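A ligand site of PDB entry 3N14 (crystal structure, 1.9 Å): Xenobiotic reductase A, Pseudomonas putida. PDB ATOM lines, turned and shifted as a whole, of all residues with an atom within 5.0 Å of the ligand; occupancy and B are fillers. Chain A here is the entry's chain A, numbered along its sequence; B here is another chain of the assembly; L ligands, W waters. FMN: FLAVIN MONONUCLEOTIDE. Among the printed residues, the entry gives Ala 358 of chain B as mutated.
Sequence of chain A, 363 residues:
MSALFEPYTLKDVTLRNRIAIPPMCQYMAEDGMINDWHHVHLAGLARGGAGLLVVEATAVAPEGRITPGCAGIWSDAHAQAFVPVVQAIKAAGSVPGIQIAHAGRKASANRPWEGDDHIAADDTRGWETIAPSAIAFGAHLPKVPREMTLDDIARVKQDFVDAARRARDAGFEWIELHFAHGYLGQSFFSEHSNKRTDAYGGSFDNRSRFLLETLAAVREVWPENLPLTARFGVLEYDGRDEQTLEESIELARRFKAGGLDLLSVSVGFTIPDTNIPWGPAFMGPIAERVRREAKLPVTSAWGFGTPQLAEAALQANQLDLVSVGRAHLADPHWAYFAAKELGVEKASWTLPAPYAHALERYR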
ATOM      1  N   PRO A  22       4.592 -23.426   3.937  1.00  0.00           N
ATOM      2  CA  PRO A  22       4.397 -24.241   5.143  1.00  0.00           C
ATOM      3  C   PRO A  22       3.619 -23.447   6.178  1.00  0.00           C
ATOM      4  O   PRO A  22       3.575 -22.215   6.097  1.00  0.00           O
ATOM      5  CB  PRO A  22       5.819 -24.498   5.618  1.00  0.00           C
ATOM      6  CG  PRO A  22       6.557 -23.248   5.195  1.00  0.00           C
ATOM      7  CD  PRO A  22       5.969 -22.914   3.841  1.00  0.00           C
ATOM      8  N   PRO A  23       3.011 -24.155   7.143  1.00  0.00           N
ATOM      9  CA  PRO A  23       2.304 -23.470   8.228  1.00  0.00           C
ATOM     10  C   PRO A  23       3.245 -22.544   9.001  1.00  0.00           C
ATOM     11  O   PRO A  23       4.347 -22.942   9.420  1.00  0.00           O
ATOM     12  CB  PRO A  23       1.850 -24.624   9.130  1.00  0.00           C
ATOM     13  CG  PRO A  23       2.741 -25.770   8.772  1.00  0.00           C
ATOM     14  CD  PRO A  23       2.982 -25.622   7.310  1.00  0.00           C
ATOM     15  N   MET A  24       2.816 -21.298   9.165  1.00  0.00           N
ATOM     16  CA  MET A  24       3.542 -20.332   9.955  1.00  0.00           C
ATOM     17  C   MET A  24       2.581 -19.569  10.872  1.00  0.00           C
ATOM     18  O   MET A  24       1.783 -18.742  10.408  1.00  0.00           O
ATOM     19  CB  MET A  24       4.289 -19.353   9.047  1.00  0.00           C
ATOM     20  CG  MET A  24       5.500 -19.970   8.366  1.00  0.00           C
ATOM     21  SD  MET A  24       6.288 -18.801   7.230  1.00  0.00           S
ATOM     22  CE  MET A  24       5.084 -18.736   5.904  1.00  0.00           C
ATOM     23  N   CYS A  25       2.659 -19.854  12.174  1.00  0.00           N
ATOM     24  CA  CYS A  25       1.850 -19.149  13.171  1.00  0.00           C
ATOM     25  C   CYS A  25       1.986 -17.628  13.045  1.00  0.00           C
ATOM     26  O   CYS A  25       3.058 -17.113  12.778  1.00  0.00           O
ATOM     27  CB  CYS A  25       2.258 -19.556  14.583  1.00  0.00           C
ATOM     28  SG  CYS A  25       1.691 -21.191  15.065  1.00  0.00           S
ATOM     29  N   TYR A  27       0.082 -15.684  15.456  1.00  0.00           N
ATOM     30  CA  TYR A  27      -0.196 -15.260  16.827  1.00  0.00           C
ATOM     31  C   TYR A  27      -1.157 -14.058  16.867  1.00  0.00           C
ATOM     32  O   TYR A  27      -1.029 -13.209  17.748  1.00  0.00           O
ATOM     33  CB  TYR A  27       1.111 -14.899  17.535  1.00  0.00           C
ATOM     34  CG  TYR A  27       2.195 -15.935  17.330  1.00  0.00           C
ATOM     35  CD1 TYR A  27       2.254 -17.062  18.131  1.00  0.00           C
ATOM     36  CD2 TYR A  27       3.133 -15.791  16.321  1.00  0.00           C
ATOM     37  CE1 TYR A  27       3.238 -18.022  17.945  1.00  0.00           C
ATOM     38  CE2 TYR A  27       4.113 -16.733  16.122  1.00  0.00           C
ATOM     39  CZ  TYR A  27       4.168 -17.846  16.943  1.00  0.00           C
ATOM     40  OH  TYR A  27       5.154 -18.780  16.730  1.00  0.00           O
ATOM     41  N   GLU A  56      -1.374 -21.982   9.276  1.00  0.00           N
ATOM     42  CA  GLU A  56      -0.625 -22.192  10.515  1.00  0.00           C
ATOM     43  C   GLU A  56      -1.212 -23.256  11.463  1.00  0.00           C
ATOM     44  O   GLU A  56      -2.412 -23.543  11.432  1.00  0.00           O
ATOM     45  CB  GLU A  56      -0.551 -20.867  11.284  1.00  0.00           C
ATOM     46  CG  GLU A  56      -1.912 -20.380  11.780  1.00  0.00           C
ATOM     47  CD  GLU A  56      -1.942 -18.876  12.060  1.00  0.00           C
ATOM     48  OE1 GLU A  56      -1.614 -18.470  13.192  1.00  0.00           O
ATOM     49  OE2 GLU A  56      -2.315 -18.113  11.146  1.00  0.00           O
ATOM     50  N   ALA A  57      -0.356 -23.793  12.324  1.00  0.00           N
ATOM     51  CA  ALA A  57      -0.747 -24.691  13.405  1.00  0.00           C
ATOM     52  C   ALA A  57      -2.029 -24.200  14.087  1.00  0.00           C
ATOM     53  O   ALA A  57      -2.019 -23.177  14.771  1.00  0.00           O
ATOM     54  CB  ALA A  57       0.345 -24.774  14.408  1.00  0.00           C
ATOM     55  N   GLN A  99      -2.796 -27.118   8.901  1.00  0.00           N
ATOM     56  CA  GLN A  99      -2.131 -27.990   9.839  1.00  0.00           C
ATOM     57  C   GLN A  99      -2.940 -27.948  11.135  1.00  0.00           C
ATOM     58  O   GLN A  99      -3.210 -26.867  11.663  1.00  0.00           O
ATOM     59  CB  GLN A  99      -0.706 -27.501  10.093  1.00  0.00           C
ATOM     60  CG  GLN A  99       0.001 -28.267  11.170  1.00  0.00           C
ATOM     61  CD  GLN A  99       1.355 -27.688  11.504  1.00  0.00           C
ATOM     62  OE1 GLN A  99       1.461 -26.597  12.062  1.00  0.00           O
ATOM     63  NE2 GLN A  99       2.417 -28.406  11.144  1.00  0.00           N
ATOM     64  N   GLU A 176      -2.724 -31.406   7.313  1.00  0.00           N
ATOM     65  CA  GLU A 176      -1.432 -31.775   7.837  1.00  0.00           C
ATOM     66  C   GLU A 176      -1.524 -31.968   9.336  1.00  0.00           C
ATOM     67  O   GLU A 176      -1.900 -31.046  10.052  1.00  0.00           O
ATOM     68  CB  GLU A 176      -0.377 -30.723   7.511  1.00  0.00           C
ATOM     69  CG  GLU A 176       1.047 -31.169   7.817  1.00  0.00           C
ATOM     70  CD  GLU A 176       2.060 -30.072   7.591  1.00  0.00           C
ATOM     71  OE1 GLU A 176       2.336 -29.755   6.417  1.00  0.00           O
ATOM     72  OE2 GLU A 176       2.566 -29.513   8.597  1.00  0.00           O
ATOM     73  N   HIS A 178       0.082 -32.227  12.899  1.00  0.00           N
ATOM     74  CA  HIS A 178       1.297 -31.698  13.488  1.00  0.00           C
ATOM     75  C   HIS A 178       1.905 -32.632  14.509  1.00  0.00           C
ATOM     76  O   HIS A 178       1.737 -32.450  15.718  1.00  0.00           O
ATOM     77  CB  HIS A 178       1.052 -30.315  14.113  1.00  0.00           C
ATOM     78  CG  HIS A 178       2.295 -29.508  14.271  1.00  0.00           C
ATOM     79  ND1 HIS A 178       3.553 -30.034  14.080  1.00  0.00           N
ATOM     80  CD2 HIS A 178       2.472 -28.206  14.598  1.00  0.00           C
ATOM     81  CE1 HIS A 178       4.460 -29.091  14.276  1.00  0.00           C
ATOM     82  NE2 HIS A 178       3.829 -27.976  14.591  1.00  0.00           N
ATOM     83  N   HIS A 181       8.077 -30.873  15.989  1.00  0.00           N
ATOM     84  CA  HIS A 181       8.536 -29.698  16.740  1.00  0.00           C
ATOM     85  C   HIS A 181       8.299 -29.735  18.255  1.00  0.00           C
ATOM     86  O   HIS A 181       8.141 -28.689  18.902  1.00  0.00           O
ATOM     87  CB  HIS A 181       7.986 -28.401  16.125  1.00  0.00           C
ATOM     88  CG  HIS A 181       8.246 -28.294  14.654  1.00  0.00           C
ATOM     89  ND1 HIS A 181       7.601 -27.369  13.848  1.00  0.00           N
ATOM     90  CD2 HIS A 181       9.068 -28.990  13.832  1.00  0.00           C
ATOM     91  CE1 HIS A 181       8.029 -27.509  12.603  1.00  0.00           C
ATOM     92  NE2 HIS A 181       8.914 -28.492  12.568  1.00  0.00           N
ATOM     93  N   ARG A 231       3.352 -33.676   9.655  1.00  0.00           N
ATOM     94  CA  ARG A 231       4.697 -33.165   9.824  1.00  0.00           C
ATOM     95  C   ARG A 231       5.304 -33.925  10.983  1.00  0.00           C
ATOM     96  O   ARG A 231       4.620 -34.219  11.962  1.00  0.00           O
ATOM     97  CB  ARG A 231       4.680 -31.659  10.111  1.00  0.00           C
ATOM     98  CG  ARG A 231       6.053 -31.018   9.876  1.00  0.00           C
ATOM     99  CD  ARG A 231       5.998 -29.480   9.744  1.00  0.00           C
ATOM    100  NE  ARG A 231       7.043 -28.964   8.858  1.00  0.00           N
ATOM    101  CZ  ARG A 231       7.354 -27.688   8.711  1.00  0.00           C
ATOM    102  NH1 ARG A 231       8.311 -27.323   7.870  1.00  0.00           N
ATOM    103  NH2 ARG A 231       6.717 -26.747   9.399  1.00  0.00           N
ATOM    104  N   ALA A 301      11.814 -28.101   4.602  1.00  0.00           N
ATOM    105  CA  ALA A 301      12.044 -26.670   4.570  1.00  0.00           C
ATOM    106  C   ALA A 301      13.312 -26.305   5.321  1.00  0.00           C
ATOM    107  O   ALA A 301      13.947 -27.145   5.965  1.00  0.00           O
ATOM    108  CB  ALA A 301      10.850 -25.916   5.146  1.00  0.00           C
ATOM    109  N   TRP A 302      13.625 -25.013   5.214  1.00  0.00           N
ATOM    110  CA  TRP A 302      14.739 -24.319   5.858  1.00  0.00           C
ATOM    111  C   TRP A 302      15.779 -23.843   4.853  1.00  0.00           C
ATOM    112  O   TRP A 302      16.736 -24.572   4.527  1.00  0.00           O
ATOM    113  CB  TRP A 302      15.413 -25.087   6.998  1.00  0.00           C
ATOM    114  CG  TRP A 302      16.364 -24.192   7.699  1.00  0.00           C
ATOM    115  CD1 TRP A 302      17.664 -23.940   7.344  1.00  0.00           C
ATOM    116  CD2 TRP A 302      16.087 -23.361   8.826  1.00  0.00           C
ATOM    117  NE1 TRP A 302      18.210 -23.007   8.196  1.00  0.00           N
ATOM    118  CE2 TRP A 302      17.267 -22.648   9.116  1.00  0.00           C
ATOM    119  CE3 TRP A 302      14.950 -23.156   9.621  1.00  0.00           C
ATOM    120  CZ2 TRP A 302      17.338 -21.742  10.185  1.00  0.00           C
ATOM    121  CZ3 TRP A 302      15.034 -22.263  10.667  1.00  0.00           C
ATOM    122  CH2 TRP A 302      16.222 -21.572  10.948  1.00  0.00           C
ATOM    123  N   GLY A 303      15.595 -22.624   4.361  1.00  0.00           N
ATOM    124  CA  GLY A 303      16.548 -22.016   3.455  1.00  0.00           C
ATOM    125  C   GLY A 303      16.289 -22.257   1.985  1.00  0.00           C
ATOM    126  O   GLY A 303      17.181 -22.066   1.163  1.00  0.00           O
ATOM    127  N   PHE A 304      15.072 -22.658   1.629  1.00  0.00           N
ATOM    128  CA  PHE A 304      14.767 -22.894   0.215  1.00  0.00           C
ATOM    129  C   PHE A 304      14.272 -21.629  -0.497  1.00  0.00           C
ATOM    130  O   PHE A 304      13.925 -21.657  -1.670  1.00  0.00           O
ATOM    131  CB  PHE A 304      13.796 -24.052   0.035  1.00  0.00           C
ATOM    132  CG  PHE A 304      14.388 -25.404   0.349  1.00  0.00           C
ATOM    133  CD1 PHE A 304      15.268 -26.007  -0.550  1.00  0.00           C
ATOM    134  CD2 PHE A 304      14.075 -26.069   1.523  1.00  0.00           C
ATOM    135  CE1 PHE A 304      15.814 -27.246  -0.273  1.00  0.00           C
ATOM    136  CE2 PHE A 304      14.622 -27.318   1.801  1.00  0.00           C
ATOM    137  CZ  PHE A 304      15.501 -27.902   0.899  1.00  0.00           C
ATOM    138  N   SER A 323       9.003 -26.423   0.510  1.00  0.00           N
ATOM    139  CA  SER A 323       8.353 -25.533   1.455  1.00  0.00           C
ATOM    140  C   SER A 323       9.203 -24.288   1.721  1.00  0.00           C
ATOM    141  O   SER A 323      10.356 -24.398   2.147  1.00  0.00           O
ATOM    142  CB  SER A 323       8.039 -26.259   2.757  1.00  0.00           C
ATOM    143  OG  SER A 323       7.005 -27.223   2.551  1.00  0.00           O
ATOM    144  N   VAL A 324       8.623 -23.119   1.467  1.00  0.00           N
ATOM    145  CA  VAL A 324       9.316 -21.823   1.603  1.00  0.00           C
ATOM    146  C   VAL A 324       8.556 -20.939   2.562  1.00  0.00           C
ATOM    147  O   VAL A 324       7.463 -20.473   2.245  1.00  0.00           O
ATOM    148  CB  VAL A 324       9.387 -21.109   0.262  1.00  0.00           C
ATOM    149  CG1 VAL A 324      10.114 -19.759   0.408  1.00  0.00           C
ATOM    150  CG2 VAL A 324      10.088 -21.997  -0.753  1.00  0.00           C
ATOM    151  N   GLY A 325       9.141 -20.692   3.738  1.00  0.00           N
ATOM    152  CA  GLY A 325       8.404 -20.080   4.825  1.00  0.00           C
ATOM    153  C   GLY A 325       8.652 -18.577   4.923  1.00  0.00           C
ATOM    154  O   GLY A 325       7.888 -17.767   4.399  1.00  0.00           O
ATOM    155  N   ARG A 326       9.749 -18.235   5.593  1.00  0.00           N
ATOM    156  CA  ARG A 326      10.088 -16.854   5.908  1.00  0.00           C
ATOM    157  C   ARG A 326      10.179 -15.939   4.674  1.00  0.00           C
ATOM    158  O   ARG A 326       9.782 -14.777   4.737  1.00  0.00           O
ATOM    159  CB  ARG A 326      11.374 -16.810   6.733  1.00  0.00           C
ATOM    160  CG  ARG A 326      11.165 -17.145   8.219  1.00  0.00           C
ATOM    161  CD  ARG A 326      12.475 -17.339   8.940  1.00  0.00           C
ATOM    162  NE  ARG A 326      13.104 -18.599   8.546  1.00  0.00           N
ATOM    163  CZ  ARG A 326      14.329 -18.970   8.890  1.00  0.00           C
ATOM    164  NH1 ARG A 326      15.087 -18.182   9.639  1.00  0.00           N
ATOM    165  NH2 ARG A 326      14.804 -20.132   8.474  1.00  0.00           N
ATOM    166  N   ALA A 327      10.698 -16.457   3.564  1.00  0.00           N
ATOM    167  CA  ALA A 327      10.783 -15.662   2.342  1.00  0.00           C
ATOM    168  C   ALA A 327       9.408 -15.165   1.894  1.00  0.00           C
ATOM    169  O   ALA A 327       9.294 -14.103   1.282  1.00  0.00           O
ATOM    170  CB  ALA A 327      11.470 -16.456   1.219  1.00  0.00           C
ATOM    171  N   LEU A 329       7.008 -14.407   4.068  1.00  0.00           N
ATOM    172  CA  LEU A 329       6.638 -13.342   4.979  1.00  0.00           C
ATOM    173  C   LEU A 329       7.315 -12.061   4.527  1.00  0.00           C
ATOM    174  O   LEU A 329       6.749 -10.983   4.648  1.00  0.00           O
ATOM    175  CB  LEU A 329       7.051 -13.675   6.409  1.00  0.00           C
ATOM    176  CG  LEU A 329       6.568 -14.987   7.041  1.00  0.00           C
ATOM    177  CD1 LEU A 329       7.235 -15.184   8.388  1.00  0.00           C
ATOM    178  CD2 LEU A 329       5.028 -15.026   7.176  1.00  0.00           C
ATOM    179  N   PRO B 354       3.856  -9.923  13.307  1.00  0.00           N
ATOM    180  CA  PRO B 354       3.849 -11.331  12.883  1.00  0.00           C
ATOM    181  C   PRO B 354       4.885 -11.619  11.794  1.00  0.00           C
ATOM    182  O   PRO B 354       5.301 -12.765  11.626  1.00  0.00           O
ATOM    183  CB  PRO B 354       2.425 -11.541  12.344  1.00  0.00           C
ATOM    184  CG  PRO B 354       1.592 -10.534  13.081  1.00  0.00           C
ATOM    185  CD  PRO B 354       2.503  -9.333  13.303  1.00  0.00           C
ATOM    186  N   HIS B 357       9.127  -9.981  13.631  1.00  0.00           N
ATOM    187  CA  HIS B 357       9.860 -10.758  14.627  1.00  0.00           C
ATOM    188  C   HIS B 357      10.585 -11.906  13.938  1.00  0.00           C
ATOM    189  O   HIS B 357      11.720 -12.215  14.267  1.00  0.00           O
ATOM    190  CB  HIS B 357       8.914 -11.274  15.726  1.00  0.00           C
ATOM    191  CG  HIS B 357       8.358 -12.643  15.455  1.00  0.00           C
ATOM    192  ND1 HIS B 357       7.205 -12.847  14.714  1.00  0.00           N
ATOM    193  CD2 HIS B 357       8.779 -13.874  15.833  1.00  0.00           C
ATOM    194  CE1 HIS B 357       6.945 -14.142  14.656  1.00  0.00           C
ATOM    195  NE2 HIS B 357       7.890 -14.784  15.328  1.00  0.00           N
ATOM    196  N   ALA B 358       9.919 -12.502  12.957  1.00  0.00           N
ATOM    197  CA  ALA B 358      10.463 -13.663  12.263  1.00  0.00           C
ATOM    198  C   ALA B 358      11.626 -13.297  11.346  1.00  0.00           C
ATOM    199  O   ALA B 358      12.470 -14.140  11.054  1.00  0.00           O
ATOM    200  CB  ALA B 358       9.363 -14.340  11.463  1.00  0.00           C
HETATM  201  N1  FMN L   1       5.933 -24.891  11.435  1.00  0.00           N
HETATM  202  C2  FMN L   1       4.876 -25.715  11.732  1.00  0.00           C
HETATM  203  O2  FMN L   1       4.993 -26.915  11.476  1.00  0.00           O
HETATM  204  N3  FMN L   1       3.774 -25.099  12.293  1.00  0.00           N
HETATM  205  C4  FMN L   1       3.721 -23.751  12.556  1.00  0.00           C
HETATM  206  O4  FMN L   1       2.699 -23.271  13.064  1.00  0.00           O
HETATM  207  C4A FMN L   1       4.765 -22.883  12.287  1.00  0.00           C
HETATM  208  N5  FMN L   1       4.799 -21.523  12.531  1.00  0.00           N
HETATM  209  C5A FMN L   1       5.916 -20.774  12.186  1.00  0.00           C
HETATM  210  C6  FMN L   1       5.963 -19.397  12.402  1.00  0.00           C
HETATM  211  C7  FMN L   1       7.067 -18.613  12.087  1.00  0.00           C
HETATM  212  C7M FMN L   1       6.775 -17.182  12.462  1.00  0.00           C
HETATM  213  C8  FMN L   1       8.123 -19.296  11.509  1.00  0.00           C
HETATM  214  C8M FMN L   1       9.293 -18.399  11.174  1.00  0.00           C
HETATM  215  C9  FMN L   1       8.070 -20.671  11.305  1.00  0.00           C
HETATM  216  C9A FMN L   1       6.986 -21.474  11.618  1.00  0.00           C
HETATM  217  N10 FMN L   1       6.973 -22.833  11.377  1.00  0.00           N
HETATM  218  C10 FMN L   1       5.852 -23.554  11.708  1.00  0.00           C
HETATM  219  C1' FMN L   1       8.175 -23.496  10.730  1.00  0.00           C
HETATM  220  C2' FMN L   1       8.055 -23.175   9.232  1.00  0.00           C
HETATM  221  O2' FMN L   1       6.967 -23.899   8.702  1.00  0.00           O
HETATM  222  C3' FMN L   1       9.301 -23.529   8.408  1.00  0.00           C
HETATM  223  O3' FMN L   1       9.586 -24.909   8.546  1.00  0.00           O
HETATM  224  C4' FMN L   1      10.520 -22.707   8.858  1.00  0.00           C
HETATM  225  O4' FMN L   1      10.254 -21.305   8.848  1.00  0.00           O
HETATM  226  C5' FMN L   1      11.780 -22.941   8.019  1.00  0.00           C
HETATM  227  O5' FMN L   1      11.554 -22.708   6.645  1.00  0.00           O
HETATM  228  P   FMN L   1      12.055 -21.321   5.973  1.00  0.00           P
HETATM  229  O1P FMN L   1      11.576 -20.179   6.841  1.00  0.00           O
HETATM  230  O2P FMN L   1      13.570 -21.264   5.959  1.00  0.00           O
HETATM  231  O3P FMN L   1      11.545 -21.236   4.554  1.00  0.00           O
HETATM  232  O   HOH W   1       9.485 -24.601  13.443  1.00  0.00           O
HETATM  233  O   HOH W   2      10.681 -25.885  10.815  1.00  0.00           O
HETATM  234  O   HOH W   3      12.172 -19.002   3.159  1.00  0.00           O
HETATM  235  O   HOH W   4      15.119 -19.004   5.430  1.00  0.00           O
HETATM  236  O   HOH W   5      12.624 -23.291   3.249  1.00  0.00           O
HETATM  237  O   HOH W   6      11.751 -20.820  11.270  1.00  0.00           O
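The side-chain carboxylate (OE2) of Glu 176 is in hydrogen-bond range of the side-chain amide nitrogen (NE2) of Gln 99 (2.8 Å). The backbone NH (N) of Ala 57 sits close to the side-chain amide oxygen (OE1) of Gln 99 (3.4 Å).
N of Cys 25 sits at hydrogen-bond distance from N5 of the ligand (2.7 Å). O2' of the ligand sits close to O of Pro 23, at 2.9 Å. N of Trp 302 is in hydrogen-bond range of O5' of the ligand. The side-chain sulfur (SG) of Cys 25 sits at hydrogen-bond distance from an oxygen (O4) of the ligand, at 3.1 Å. The backbone NH of Arg 326 lies within hydrogen-bond range of an oxygen (O1P) of the ligand (2.9 Å). The backbone NH of Ala 57 lies close to an oxygen (O4) of the ligand, 3.2 Å away. The side-chain amide oxygen (OE1) of Gln 99 sits at hydrogen-bond distance from a nitrogen (N3) of the ligand (2.8 Å). NE of Arg 326 is in salt-bridge range of O1P of the ligand (2.8 Å). NH2 of Arg 231 is in hydrogen-bond range of O2 of the ligand, 2.7 Å away. N of Gly 325 is in hydrogen-bond range of O3P of the ligand (2.6 Å). N of Gly 303 lies within hydrogen-bond range of O2P of the ligand, 2.9 Å away. A ring nitrogen (NE2) of His 178 is in hydrogen-bond range of an oxygen (O2) of the ligand (3.5 Å).
Water W3 bridges an oxygen (O3P) of the ligand (2.7 Å) and the backbone NH (N) of Ala 327 (3.0 Å). Water W4 bridges O2P of the ligand (2.8 Å) and NH2 of Arg 326 (3.3 Å).
Merely in contact with the ligand: Met 24 (3.1 Å), His 181 (3.3 Å), Pro 22 (3.3 Å), Val 324 (3.6 Å), Ala 301 (3.6 Å), His 357 of chain B (3.8 Å) and Ala 358 of chain B (3.97 Å). Hydrophobic or aromatic side chains within 4 Å of the ligand: Pro 22, Pro 23, Met 24, Ala 57, His 178, His 181, Ala 301, Trp 302, His 357 of chain B and Ala 358 of chain B. Of the 25 residues printed, 17 come within 4 Å of the ligand.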
